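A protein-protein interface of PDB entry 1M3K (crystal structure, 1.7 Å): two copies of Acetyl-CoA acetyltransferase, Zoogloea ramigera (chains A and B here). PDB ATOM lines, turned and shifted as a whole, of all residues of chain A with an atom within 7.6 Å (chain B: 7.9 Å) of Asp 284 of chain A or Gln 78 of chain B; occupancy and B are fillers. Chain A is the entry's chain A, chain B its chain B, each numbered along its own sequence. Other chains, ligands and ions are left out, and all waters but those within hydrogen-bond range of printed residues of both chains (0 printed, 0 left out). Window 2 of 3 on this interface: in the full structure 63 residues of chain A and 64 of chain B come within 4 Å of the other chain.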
ATOM      1  N   ASP A 150     -18.446   4.290  18.232  1.00  0.00           N
ATOM      2  CA  ASP A 150     -18.826   3.572  19.473  1.00  0.00           C
ATOM      3  C   ASP A 150     -17.729   3.889  20.408  1.00  0.00           C
ATOM      4  O   ASP A 150     -16.541   3.768  20.065  1.00  0.00           O
ATOM      5  CB  ASP A 150     -18.906   2.064  19.297  1.00  0.00           C
ATOM      6  CG  ASP A 150     -19.390   1.378  20.558  1.00  0.00           C
ATOM      7  OD1 ASP A 150     -20.629   1.437  20.878  1.00  0.00           O
ATOM      8  OD2 ASP A 150     -18.574   0.794  21.254  1.00  0.00           O
ATOM      9  N   PHE A 152     -16.860   2.176  23.155  1.00  0.00           N
ATOM     10  CA  PHE A 152     -16.228   0.968  23.755  1.00  0.00           C
ATOM     11  C   PHE A 152     -15.300   0.190  22.817  1.00  0.00           C
ATOM     12  O   PHE A 152     -14.253  -0.383  23.228  1.00  0.00           O
ATOM     13  CB  PHE A 152     -17.386   0.089  24.267  1.00  0.00           C
ATOM     14  CG  PHE A 152     -18.309   0.823  25.097  1.00  0.00           C
ATOM     15  CD1 PHE A 152     -17.906   1.296  26.338  1.00  0.00           C
ATOM     16  CD2 PHE A 152     -19.564   1.218  24.627  1.00  0.00           C
ATOM     17  CE1 PHE A 152     -18.791   2.094  27.102  1.00  0.00           C
ATOM     18  CE2 PHE A 152     -20.429   2.015  25.384  1.00  0.00           C
ATOM     19  CZ  PHE A 152     -20.030   2.453  26.630  1.00  0.00           C
ATOM     20  N   TYR A 153     -15.640   0.159  21.551  1.00  0.00           N
ATOM     21  CA  TYR A 153     -14.953  -0.609  20.556  1.00  0.00           C
ATOM     22  C   TYR A 153     -14.176   0.256  19.570  1.00  0.00           C
ATOM     23  O   TYR A 153     -13.419  -0.272  18.793  1.00  0.00           O
ATOM     24  CB  TYR A 153     -15.894  -1.560  19.842  1.00  0.00           C
ATOM     25  CG  TYR A 153     -16.382  -2.631  20.755  1.00  0.00           C
ATOM     26  CD1 TYR A 153     -15.495  -3.584  21.233  1.00  0.00           C
ATOM     27  CD2 TYR A 153     -17.689  -2.658  21.222  1.00  0.00           C
ATOM     28  CE1 TYR A 153     -15.893  -4.556  22.104  1.00  0.00           C
ATOM     29  CE2 TYR A 153     -18.114  -3.646  22.119  1.00  0.00           C
ATOM     30  CZ  TYR A 153     -17.171  -4.606  22.554  1.00  0.00           C
ATOM     31  OH  TYR A 153     -17.504  -5.629  23.423  1.00  0.00           O
ATOM     32  N   TYR A 155     -14.941   1.902  16.896  1.00  0.00           N
ATOM     33  CA  TYR A 155     -15.332   1.892  15.478  1.00  0.00           C
ATOM     34  C   TYR A 155     -16.642   2.546  15.207  1.00  0.00           C
ATOM     35  O   TYR A 155     -17.404   2.789  16.103  1.00  0.00           O
ATOM     36  CB  TYR A 155     -15.294   0.472  14.845  1.00  0.00           C
ATOM     37  CG  TYR A 155     -15.945  -0.723  15.563  1.00  0.00           C
ATOM     38  CD1 TYR A 155     -17.306  -0.733  15.931  1.00  0.00           C
ATOM     39  CD2 TYR A 155     -15.205  -1.869  15.820  1.00  0.00           C
ATOM     40  CE1 TYR A 155     -17.870  -1.865  16.540  1.00  0.00           C
ATOM     41  CE2 TYR A 155     -15.769  -3.003  16.412  1.00  0.00           C
ATOM     42  CZ  TYR A 155     -17.097  -2.995  16.770  1.00  0.00           C
ATOM     43  OH  TYR A 155     -17.634  -4.111  17.359  1.00  0.00           O
ATOM     44  N   THR A 160     -20.923  -1.806  13.455  1.00  0.00           N
ATOM     45  CA  THR A 160     -21.956  -2.552  14.184  1.00  0.00           C
ATOM     46  C   THR A 160     -22.977  -3.093  13.213  1.00  0.00           C
ATOM     47  O   THR A 160     -23.449  -4.209  13.353  1.00  0.00           O
ATOM     48  CB  THR A 160     -22.695  -1.724  15.274  1.00  0.00           C
ATOM     49  OG1 THR A 160     -23.665  -0.811  14.689  1.00  0.00           O
ATOM     50  CG2 THR A 160     -21.683  -0.900  16.152  1.00  0.00           C
ATOM     51  N   ASN A 163     -21.547  -6.174  11.773  1.00  0.00           N
ATOM     52  CA  ASN A 163     -21.653  -7.261  12.762  1.00  0.00           C
ATOM     53  C   ASN A 163     -23.059  -7.900  12.685  1.00  0.00           C
ATOM     54  O   ASN A 163     -23.221  -9.125  12.762  1.00  0.00           O
ATOM     55  CB  ASN A 163     -21.467  -6.726  14.169  1.00  0.00           C
ATOM     56  CG  ASN A 163     -20.065  -6.326  14.478  1.00  0.00           C
ATOM     57  OD1 ASN A 163     -19.081  -6.795  13.848  1.00  0.00           O
ATOM     58  ND2 ASN A 163     -19.930  -5.467  15.490  1.00  0.00           N
ATOM     59  N   VAL A 164     -24.055  -7.055  12.561  1.00  0.00           N
ATOM     60  CA  VAL A 164     -25.454  -7.503  12.436  1.00  0.00           C
ATOM     61  C   VAL A 164     -25.695  -8.226  11.122  1.00  0.00           C
ATOM     62  O   VAL A 164     -26.313  -9.292  11.118  1.00  0.00           O
ATOM     63  CB  VAL A 164     -26.425  -6.354  12.647  1.00  0.00           C
ATOM     64  CG1 VAL A 164     -27.865  -6.750  12.235  1.00  0.00           C
ATOM     65  CG2 VAL A 164     -26.396  -5.846  14.106  1.00  0.00           C
ATOM     66  N   VAL A 281     -34.498  -0.411  26.360  1.00  0.00           N
ATOM     67  CA  VAL A 281     -33.702  -1.594  26.760  1.00  0.00           C
ATOM     68  C   VAL A 281     -32.297  -1.519  26.161  1.00  0.00           C
ATOM     69  O   VAL A 281     -32.106  -0.946  25.086  1.00  0.00           O
ATOM     70  CB  VAL A 281     -34.469  -2.932  26.387  1.00  0.00           C
ATOM     71  CG1 VAL A 281     -33.823  -4.138  26.860  1.00  0.00           C
ATOM     72  CG2 VAL A 281     -35.827  -2.905  27.010  1.00  0.00           C
ATOM     73  N   GLY A 282     -31.300  -2.107  26.858  1.00  0.00           N
ATOM     74  CA  GLY A 282     -29.966  -2.218  26.336  1.00  0.00           C
ATOM     75  C   GLY A 282     -29.732  -3.532  25.583  1.00  0.00           C
ATOM     76  O   GLY A 282     -30.363  -4.607  25.830  1.00  0.00           O
ATOM     77  N   VAL A 283     -28.721  -3.477  24.703  1.00  0.00           N
ATOM     78  CA  VAL A 283     -28.130  -4.674  24.060  1.00  0.00           C
ATOM     79  C   VAL A 283     -26.611  -4.438  23.997  1.00  0.00           C
ATOM     80  O   VAL A 283     -26.139  -3.349  24.411  1.00  0.00           O
ATOM     81  CB  VAL A 283     -28.647  -4.853  22.630  1.00  0.00           C
ATOM     82  CG1 VAL A 283     -30.111  -5.028  22.644  1.00  0.00           C
ATOM     83  CG2 VAL A 283     -28.317  -3.634  21.769  1.00  0.00           C
ATOM     84  N   ASP A 284     -25.882  -5.414  23.466  1.00  0.00           N
ATOM     85  CA  ASP A 284     -24.419  -5.298  23.324  1.00  0.00           C
ATOM     86  C   ASP A 284     -24.093  -4.137  22.347  1.00  0.00           C
ATOM     87  O   ASP A 284     -24.672  -4.062  21.266  1.00  0.00           O
ATOM     88  CB  ASP A 284     -23.854  -6.575  22.790  1.00  0.00           C
ATOM     89  CG  ASP A 284     -22.375  -6.675  23.017  1.00  0.00           C
ATOM     90  OD1 ASP A 284     -21.625  -5.950  22.360  1.00  0.00           O
ATOM     91  OD2 ASP A 284     -21.892  -7.421  23.895  1.00  0.00           O
ATOM     92  N   PRO A 285     -23.203  -3.252  22.703  1.00  0.00           N
ATOM     93  CA  PRO A 285     -22.851  -2.189  21.752  1.00  0.00           C
ATOM     94  C   PRO A 285     -22.489  -2.734  20.339  1.00  0.00           C
ATOM     95  O   PRO A 285     -22.719  -2.057  19.345  1.00  0.00           O
ATOM     96  CB  PRO A 285     -21.586  -1.586  22.367  1.00  0.00           C
ATOM     97  CG  PRO A 285     -21.754  -1.828  23.916  1.00  0.00           C
ATOM     98  CD  PRO A 285     -22.441  -3.171  23.976  1.00  0.00           C
ATOM     99  N   LYS A 286     -21.852  -3.894  20.288  1.00  0.00           N
ATOM    100  CA  LYS A 286     -21.380  -4.473  18.995  1.00  0.00           C
ATOM    101  C   LYS A 286     -22.494  -4.711  17.985  1.00  0.00           C
ATOM    102  O   LYS A 286     -22.281  -4.726  16.787  1.00  0.00           O
ATOM    103  CB  LYS A 286     -20.713  -5.805  19.249  1.00  0.00           C
ATOM    104  CG  LYS A 286     -19.318  -5.691  19.770  1.00  0.00           C
ATOM    105  CD  LYS A 286     -18.580  -7.051  19.692  1.00  0.00           C
ATOM    106  CE  LYS A 286     -19.280  -8.139  20.528  1.00  0.00           C
ATOM    107  NZ  LYS A 286     -19.487  -7.723  21.950  1.00  0.00           N
ATOM    108  N   VAL A 287     -23.701  -4.898  18.498  1.00  0.00           N
ATOM    109  CA  VAL A 287     -24.895  -5.129  17.701  1.00  0.00           C
ATOM    110  C   VAL A 287     -26.035  -4.205  18.108  1.00  0.00           C
ATOM    111  O   VAL A 287     -27.192  -4.638  18.176  1.00  0.00           O
ATOM    112  CB  VAL A 287     -25.329  -6.649  17.799  1.00  0.00           C
ATOM    113  CG1 VAL A 287     -24.406  -7.529  16.984  1.00  0.00           C
ATOM    114  CG2 VAL A 287     -25.513  -7.064  19.226  1.00  0.00           C
ATOM    115  N   MET A 288     -25.717  -2.907  18.232  1.00  0.00           N
ATOM    116  CA  MET A 288     -26.616  -1.899  18.713  1.00  0.00           C
ATOM    117  C   MET A 288     -27.873  -1.787  17.863  1.00  0.00           C
ATOM    118  O   MET A 288     -28.908  -1.417  18.359  1.00  0.00           O
ATOM    119  CB  MET A 288     -25.923  -0.547  18.798  1.00  0.00           C
ATOM    120  CG  MET A 288     -25.594   0.089  17.480  1.00  0.00           C
ATOM    121  SD  MET A 288     -26.873   1.152  16.868  1.00  0.00           S
ATOM    122  CE  MET A 288     -26.379   1.284  15.226  1.00  0.00           C
ATOM    123  N   GLY A 289     -27.747  -2.103  16.565  1.00  0.00           N
ATOM    124  CA  GLY A 289     -28.886  -2.043  15.637  1.00  0.00           C
ATOM    125  C   GLY A 289     -29.987  -3.030  15.970  1.00  0.00           C
ATOM    126  O   GLY A 289     -31.115  -2.914  15.470  1.00  0.00           O
ATOM    127  N   THR A 290     -29.642  -3.972  16.851  1.00  0.00           N
ATOM    128  CA  THR A 290     -30.646  -4.894  17.420  1.00  0.00           C
ATOM    129  C   THR A 290     -31.513  -4.382  18.527  1.00  0.00           C
ATOM    130  O   THR A 290     -32.553  -5.009  18.817  1.00  0.00           O
ATOM    131  CB  THR A 290     -30.069  -6.203  17.873  1.00  0.00           C
ATOM    132  OG1 THR A 290     -29.201  -5.994  18.979  1.00  0.00           O
ATOM    133  CG2 THR A 290     -29.314  -6.896  16.784  1.00  0.00           C
ATOM    134  N   GLY A 291     -31.216  -3.193  19.052  1.00  0.00           N
ATOM    135  CA  GLY A 291     -32.010  -2.594  20.111  1.00  0.00           C
ATOM    136  C   GLY A 291     -33.510  -2.593  19.952  1.00  0.00           C
ATOM    137  O   GLY A 291     -34.224  -2.758  20.890  1.00  0.00           O
ATOM    138  N   ILE A 379     -29.984   2.488  18.913  1.00  0.00           N
ATOM    139  CA  ILE A 379     -29.221   3.501  19.609  1.00  0.00           C
ATOM    140  C   ILE A 379     -27.742   3.088  19.828  1.00  0.00           C
ATOM    141  O   ILE A 379     -27.506   2.029  20.364  1.00  0.00           O
ATOM    142  CB  ILE A 379     -29.902   3.804  20.980  1.00  0.00           C
ATOM    143  CG1 ILE A 379     -31.383   4.172  20.816  1.00  0.00           C
ATOM    144  CG2 ILE A 379     -29.181   4.972  21.696  1.00  0.00           C
ATOM    145  CD1 ILE A 379     -32.132   4.315  22.167  1.00  0.00           C
ATOM    146  N   GLY A 380     -26.792   3.962  19.461  1.00  0.00           N
ATOM    147  CA  GLY A 380     -25.380   3.690  19.544  1.00  0.00           C
ATOM    148  C   GLY A 380     -25.073   3.424  20.986  1.00  0.00           C
ATOM    149  O   GLY A 380     -25.729   3.916  21.885  1.00  0.00           O
ATOM    150  N   GLY A 381     -24.090   2.583  21.241  1.00  0.00           N
ATOM    151  CA  GLY A 381     -23.857   2.195  22.591  1.00  0.00           C
ATOM    152  C   GLY A 381     -24.708   1.043  23.071  1.00  0.00           C
ATOM    153  O   GLY A 381     -24.490   0.567  24.216  1.00  0.00           O
ATOM    154  N   GLY A 382     -25.637   0.564  22.220  1.00  0.00           N
ATOM    155  CA  GLY A 382     -26.375  -0.632  22.567  1.00  0.00           C
ATOM    156  C   GLY A 382     -27.675  -0.385  23.310  1.00  0.00           C
ATOM    157  O   GLY A 382     -27.876  -0.867  24.406  1.00  0.00           O
ATOM    158  N   MET A 383     -28.599   0.330  22.703  1.00  0.00           N
ATOM    159  CA  MET A 383     -29.920   0.423  23.262  1.00  0.00           C
ATOM    160  C   MET A 383     -30.992   0.410  22.196  1.00  0.00           C
ATOM    161  O   MET A 383     -30.748   0.563  21.006  1.00  0.00           O
ATOM    162  CB  MET A 383     -30.037   1.676  24.176  1.00  0.00           C
ATOM    163  CG  MET A 383     -29.065   1.714  25.352  1.00  0.00           C
ATOM    164  SD  MET A 383     -29.107   3.255  26.225  1.00  0.00           S
ATOM    165  CE  MET A 383     -27.982   4.155  25.195  1.00  0.00           C
ATOM    166  N   ASN B  50     -31.517  -0.334  36.658  1.00  0.00           N
ATOM    167  CA  ASN B  50     -32.268  -0.255  35.374  1.00  0.00           C
ATOM    168  C   ASN B  50     -31.727   0.852  34.473  1.00  0.00           C
ATOM    169  O   ASN B  50     -31.569   0.638  33.252  1.00  0.00           O
ATOM    170  CB  ASN B  50     -33.782  -0.099  35.622  1.00  0.00           C
ATOM    171  CG  ASN B  50     -34.372  -1.215  36.428  1.00  0.00           C
ATOM    172  OD1 ASN B  50     -34.858  -0.977  37.495  1.00  0.00           O
ATOM    173  ND2 ASN B  50     -34.223  -2.488  35.980  1.00  0.00           N
ATOM    174  N   ARG B  68     -23.503   6.534  29.334  1.00  0.00           N
ATOM    175  CA  ARG B  68     -23.387   5.100  29.046  1.00  0.00           C
ATOM    176  C   ARG B  68     -21.984   4.657  29.286  1.00  0.00           C
ATOM    177  O   ARG B  68     -21.722   3.571  29.792  1.00  0.00           O
ATOM    178  CB  ARG B  68     -23.834   4.853  27.615  1.00  0.00           C
ATOM    179  CG  ARG B  68     -23.759   3.385  27.162  1.00  0.00           C
ATOM    180  CD  ARG B  68     -24.697   2.420  27.838  1.00  0.00           C
ATOM    181  NE  ARG B  68     -24.859   1.208  27.035  1.00  0.00           N
ATOM    182  CZ  ARG B  68     -25.653   0.198  27.371  1.00  0.00           C
ATOM    183  NH1 ARG B  68     -26.262   0.156  28.549  1.00  0.00           N
ATOM    184  NH2 ARG B  68     -25.838  -0.775  26.541  1.00  0.00           N
ATOM    185  N   ALA B  71     -21.709   4.360  33.117  1.00  0.00           N
ATOM    186  CA  ALA B  71     -22.407   3.111  33.528  1.00  0.00           C
ATOM    187  C   ALA B  71     -21.650   1.845  33.217  1.00  0.00           C
ATOM    188  O   ALA B  71     -21.462   1.012  34.080  1.00  0.00           O
ATOM    189  CB  ALA B  71     -23.765   3.080  32.945  1.00  0.00           C
ATOM    190  N   MET B  72     -21.145   1.719  31.996  1.00  0.00           N
ATOM    191  CA  MET B  72     -20.418   0.508  31.575  1.00  0.00           C
ATOM    192  C   MET B  72     -19.122   0.328  32.372  1.00  0.00           C
ATOM    193  O   MET B  72     -18.754  -0.813  32.727  1.00  0.00           O
ATOM    194  CB  MET B  72     -20.203   0.550  30.079  1.00  0.00           C
ATOM    195  CG  MET B  72     -21.552   0.474  29.300  1.00  0.00           C
ATOM    196  SD  MET B  72     -22.236  -1.269  29.178  1.00  0.00           S
ATOM    197  CE  MET B  72     -21.205  -1.853  27.949  1.00  0.00           C
ATOM    198  N   GLY B  75     -19.779  -1.277  35.632  1.00  0.00           N
ATOM    199  CA  GLY B  75     -20.224  -2.676  35.720  1.00  0.00           C
ATOM    200  C   GLY B  75     -21.716  -2.782  35.584  1.00  0.00           C
ATOM    201  O   GLY B  75     -22.240  -3.880  35.669  1.00  0.00           O
ATOM    202  N   VAL B  76     -22.406  -1.674  35.226  1.00  0.00           N
ATOM    203  CA  VAL B  76     -23.816  -1.732  34.982  1.00  0.00           C
ATOM    204  C   VAL B  76     -23.942  -2.496  33.658  1.00  0.00           C
ATOM    205  O   VAL B  76     -23.205  -2.189  32.686  1.00  0.00           O
ATOM    206  CB  VAL B  76     -24.460  -0.286  34.859  1.00  0.00           C
ATOM    207  CG1 VAL B  76     -25.856  -0.344  34.458  1.00  0.00           C
ATOM    208  CG2 VAL B  76     -24.238   0.480  36.229  1.00  0.00           C
ATOM    209  N   PRO B  77     -24.828  -3.493  33.616  1.00  0.00           N
ATOM    210  CA  PRO B  77     -24.802  -4.423  32.492  1.00  0.00           C
ATOM    211  C   PRO B  77     -25.382  -3.789  31.257  1.00  0.00           C
ATOM    212  O   PRO B  77     -26.136  -2.803  31.261  1.00  0.00           O
ATOM    213  CB  PRO B  77     -25.668  -5.581  32.968  1.00  0.00           C
ATOM    214  CG  PRO B  77     -26.714  -4.902  33.781  1.00  0.00           C
ATOM    215  CD  PRO B  77     -25.925  -3.818  34.564  1.00  0.00           C
ATOM    216  N   GLN B  78     -25.032  -4.377  30.128  1.00  0.00           N
ATOM    217  CA  GLN B  78     -25.499  -3.792  28.819  1.00  0.00           C
ATOM    218  C   GLN B  78     -26.956  -3.751  28.658  1.00  0.00           C
ATOM    219  O   GLN B  78     -27.497  -2.922  27.838  1.00  0.00           O
ATOM    220  CB  GLN B  78     -24.866  -4.572  27.633  1.00  0.00           C
ATOM    221  CG  GLN B  78     -25.412  -6.018  27.478  1.00  0.00           C
ATOM    222  CD  GLN B  78     -24.650  -6.925  26.513  1.00  0.00           C
ATOM    223  OE1 GLN B  78     -25.248  -7.878  25.935  1.00  0.00           O
ATOM    224  NE2 GLN B  78     -23.361  -6.737  26.406  1.00  0.00           N
ATOM    225  N   GLU B  79     -27.680  -4.548  29.448  1.00  0.00           N
ATOM    226  CA  GLU B  79     -29.142  -4.502  29.279  1.00  0.00           C
ATOM    227  C   GLU B  79     -29.858  -3.349  29.923  1.00  0.00           C
ATOM    228  O   GLU B  79     -31.025  -3.102  29.604  1.00  0.00           O
ATOM    229  CB  GLU B  79     -29.757  -5.804  29.800  1.00  0.00           C
ATOM    230  CG  GLU B  79     -29.356  -7.043  29.025  1.00  0.00           C
ATOM    231  CD  GLU B  79     -28.013  -7.674  29.451  1.00  0.00           C
ATOM    232  OE1 GLU B  79     -27.430  -7.217  30.438  1.00  0.00           O
ATOM    233  OE2 GLU B  79     -27.547  -8.660  28.825  1.00  0.00           O
ATOM    234  N   ALA B  80     -29.188  -2.646  30.830  1.00  0.00           N
ATOM    235  CA  ALA B  80     -29.638  -1.380  31.381  1.00  0.00           C
ATOM    236  C   ALA B  80     -29.513  -0.287  30.317  1.00  0.00           C
ATOM    237  O   ALA B  80     -29.039  -0.518  29.187  1.00  0.00           O
ATOM    238  CB  ALA B  80     -28.742  -1.039  32.561  1.00  0.00           C
ATOM    239  N   THR B  81     -29.970   0.889  30.644  1.00  0.00           N
ATOM    240  CA  THR B  81     -29.879   2.031  29.723  1.00  0.00           C
ATOM    241  C   THR B  81     -29.259   3.215  30.430  1.00  0.00           C
ATOM    242  O   THR B  81     -29.128   3.211  31.649  1.00  0.00           O
ATOM    243  CB  THR B  81     -31.244   2.435  29.136  1.00  0.00           C
ATOM    244  OG1 THR B  81     -32.269   2.630  30.162  1.00  0.00           O
ATOM    245  CG2 THR B  81     -31.749   1.290  28.242  1.00  0.00           C
ATOM    246  N   ALA B  82     -28.924   4.258  29.697  1.00  0.00           N
ATOM    247  CA  ALA B  82     -28.229   5.426  30.312  1.00  0.00           C
ATOM    248  C   ALA B  82     -28.406   6.554  29.334  1.00  0.00           C
ATOM    249  O   ALA B  82     -28.352   6.351  28.143  1.00  0.00           O
ATOM    250  CB  ALA B  82     -26.786   5.192  30.463  1.00  0.00           C
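The side-chain amide nitrogen (NE2) of Gln 78 of chain B lies within hydrogen-bond range of the side-chain carboxylate (OD2) of Asp 284 of chain A (3.0 Å). The side-chain sulfur of Met 383 of chain A lies within hydrogen-bond range of the backbone NH of Ala 82 of chain B (3.6 Å). The backbone carbonyl oxygen (O) of Gln 78 of chain B is in hydrogen-bond range of the backbone NH (N) of Val 283 of chain A, at 3.4 Å. O of Gly 381 of chain A sits at hydrogen-bond distance from NE of Arg 68 of chain B, at 2.9 Å. The backbone carbonyl oxygen of Gly 382 of chain A is in hydrogen-bond range of the guanidinium group of Arg 68 of chain B (3.0 Å). N of Gly 282 of chain A is in hydrogen-bond range of O of Glu 79 of chain B (2.9 Å). The backbone carbonyl oxygen (O) of Val 283 of chain A is in hydrogen-bond range of the guanidinium group (NH2) of Arg 68 of chain B (3.4 Å).
The side-chain carboxylate of Asp 284 of chain A lies within salt-bridge range of the side-chain amino group of Lys 286 of chain A (2.8 Å). O of Gln 78 of chain B is in hydrogen-bond range of NH2 of Arg 68 of chain B (3.0 Å). The backbone NH (N) of Val 283 of chain A sits at hydrogen-bond distance from the backbone carbonyl oxygen (O) of Gly 382 of chain A, at 2.8 Å. The backbone NH of Thr 81 of chain B is in hydrogen-bond range of the backbone carbonyl oxygen of Asn 50 of chain B (3.1 Å). OD2 of Asp 150 of chain A sits at hydrogen-bond distance from N of Phe 152 of chain A (2.9 Å). The backbone carbonyl oxygen (O) of Ala 80 of chain B lies within hydrogen-bond range of the guanidinium group (NH1) of Arg 68 of chain B (2.9 Å).
Among the printed residues, merely in contact across the chains: Gly 282 of chain A with Gln 78 of chain B (3.0 Å), Gly 282 of chain A with Ala 80 of chain B (3.4 Å), Val 281 of chain A with Thr 81 of chain B (3.5 Å), Phe 152 of chain A with Met 72 of chain B (3.6 Å), Gly 282 of chain A with Thr 81 of chain B (3.7 Å), Met 383 of chain A with Thr 81 of chain B (3.7 Å), Phe 152 of chain A with Arg 68 of chain B (3.8 Å) and Val 281 of chain A with Glu 79 of chain B (3.997 Å).
Of chain B, only Gln 78 comes within 4 Å of Asp 284 of chain A. Printed residues of chain A within 4 Å of Gln 78 of chain B: Gly 282, Val 283 and Asp 284. No residue of chain B comes within 4 Å of Pro 285 of chain A. Of the printed residues of chain B, Gly 382 of chain A touches Arg 68 (3.0 Å). Of the printed residues of chain B, Gly 282 of chain A touches Gln 78, Glu 79, Ala 80 and Thr 81. Thr 290 of chain A touches none of the printed residues of chain B. Val 164 of chain A touches none of the printed residues of chain B. The nearest printed residue of chain A that does not touch Gln 78 of chain B is Gly 382 of chain A (4.02 Å). The nearest printed residue of chain B that does not touch Val 283 of chain A is Glu 79 of chain B (4.7 Å).
Of the 12 printed residues of chain B, 7 touch a printed residue of chain A. Hydrophobic or aromatic side chains of chain B within 4 Å of the printed part of chain A: Met 72. Along chain B the printed residues that touch a printed residue of chain A span positions 68 to 82. Of the 23 printed residues of chain A, 8 touch a printed residue of chain B. Printed residues of chain A that touch a printed residue of chain B: Phe 152, Val 281, Gly 282, Val 283, Asp 284, Gly 381, Gly 382 and Met 383. Along chain A the printed residues that touch a printed residue of chain B span positions 152 to 383. Among the printed residues, 15 pairs touch across the chains. Among the printed residues, no Asp or Glu carboxylate lies within 4 Å of a Lys or Arg side-chain nitrogen of the other chain.
No position is printed for both chains. Of the 15 pairs that touch across the chains among the printed residues, none has its exchanged pair printed and touching as well.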
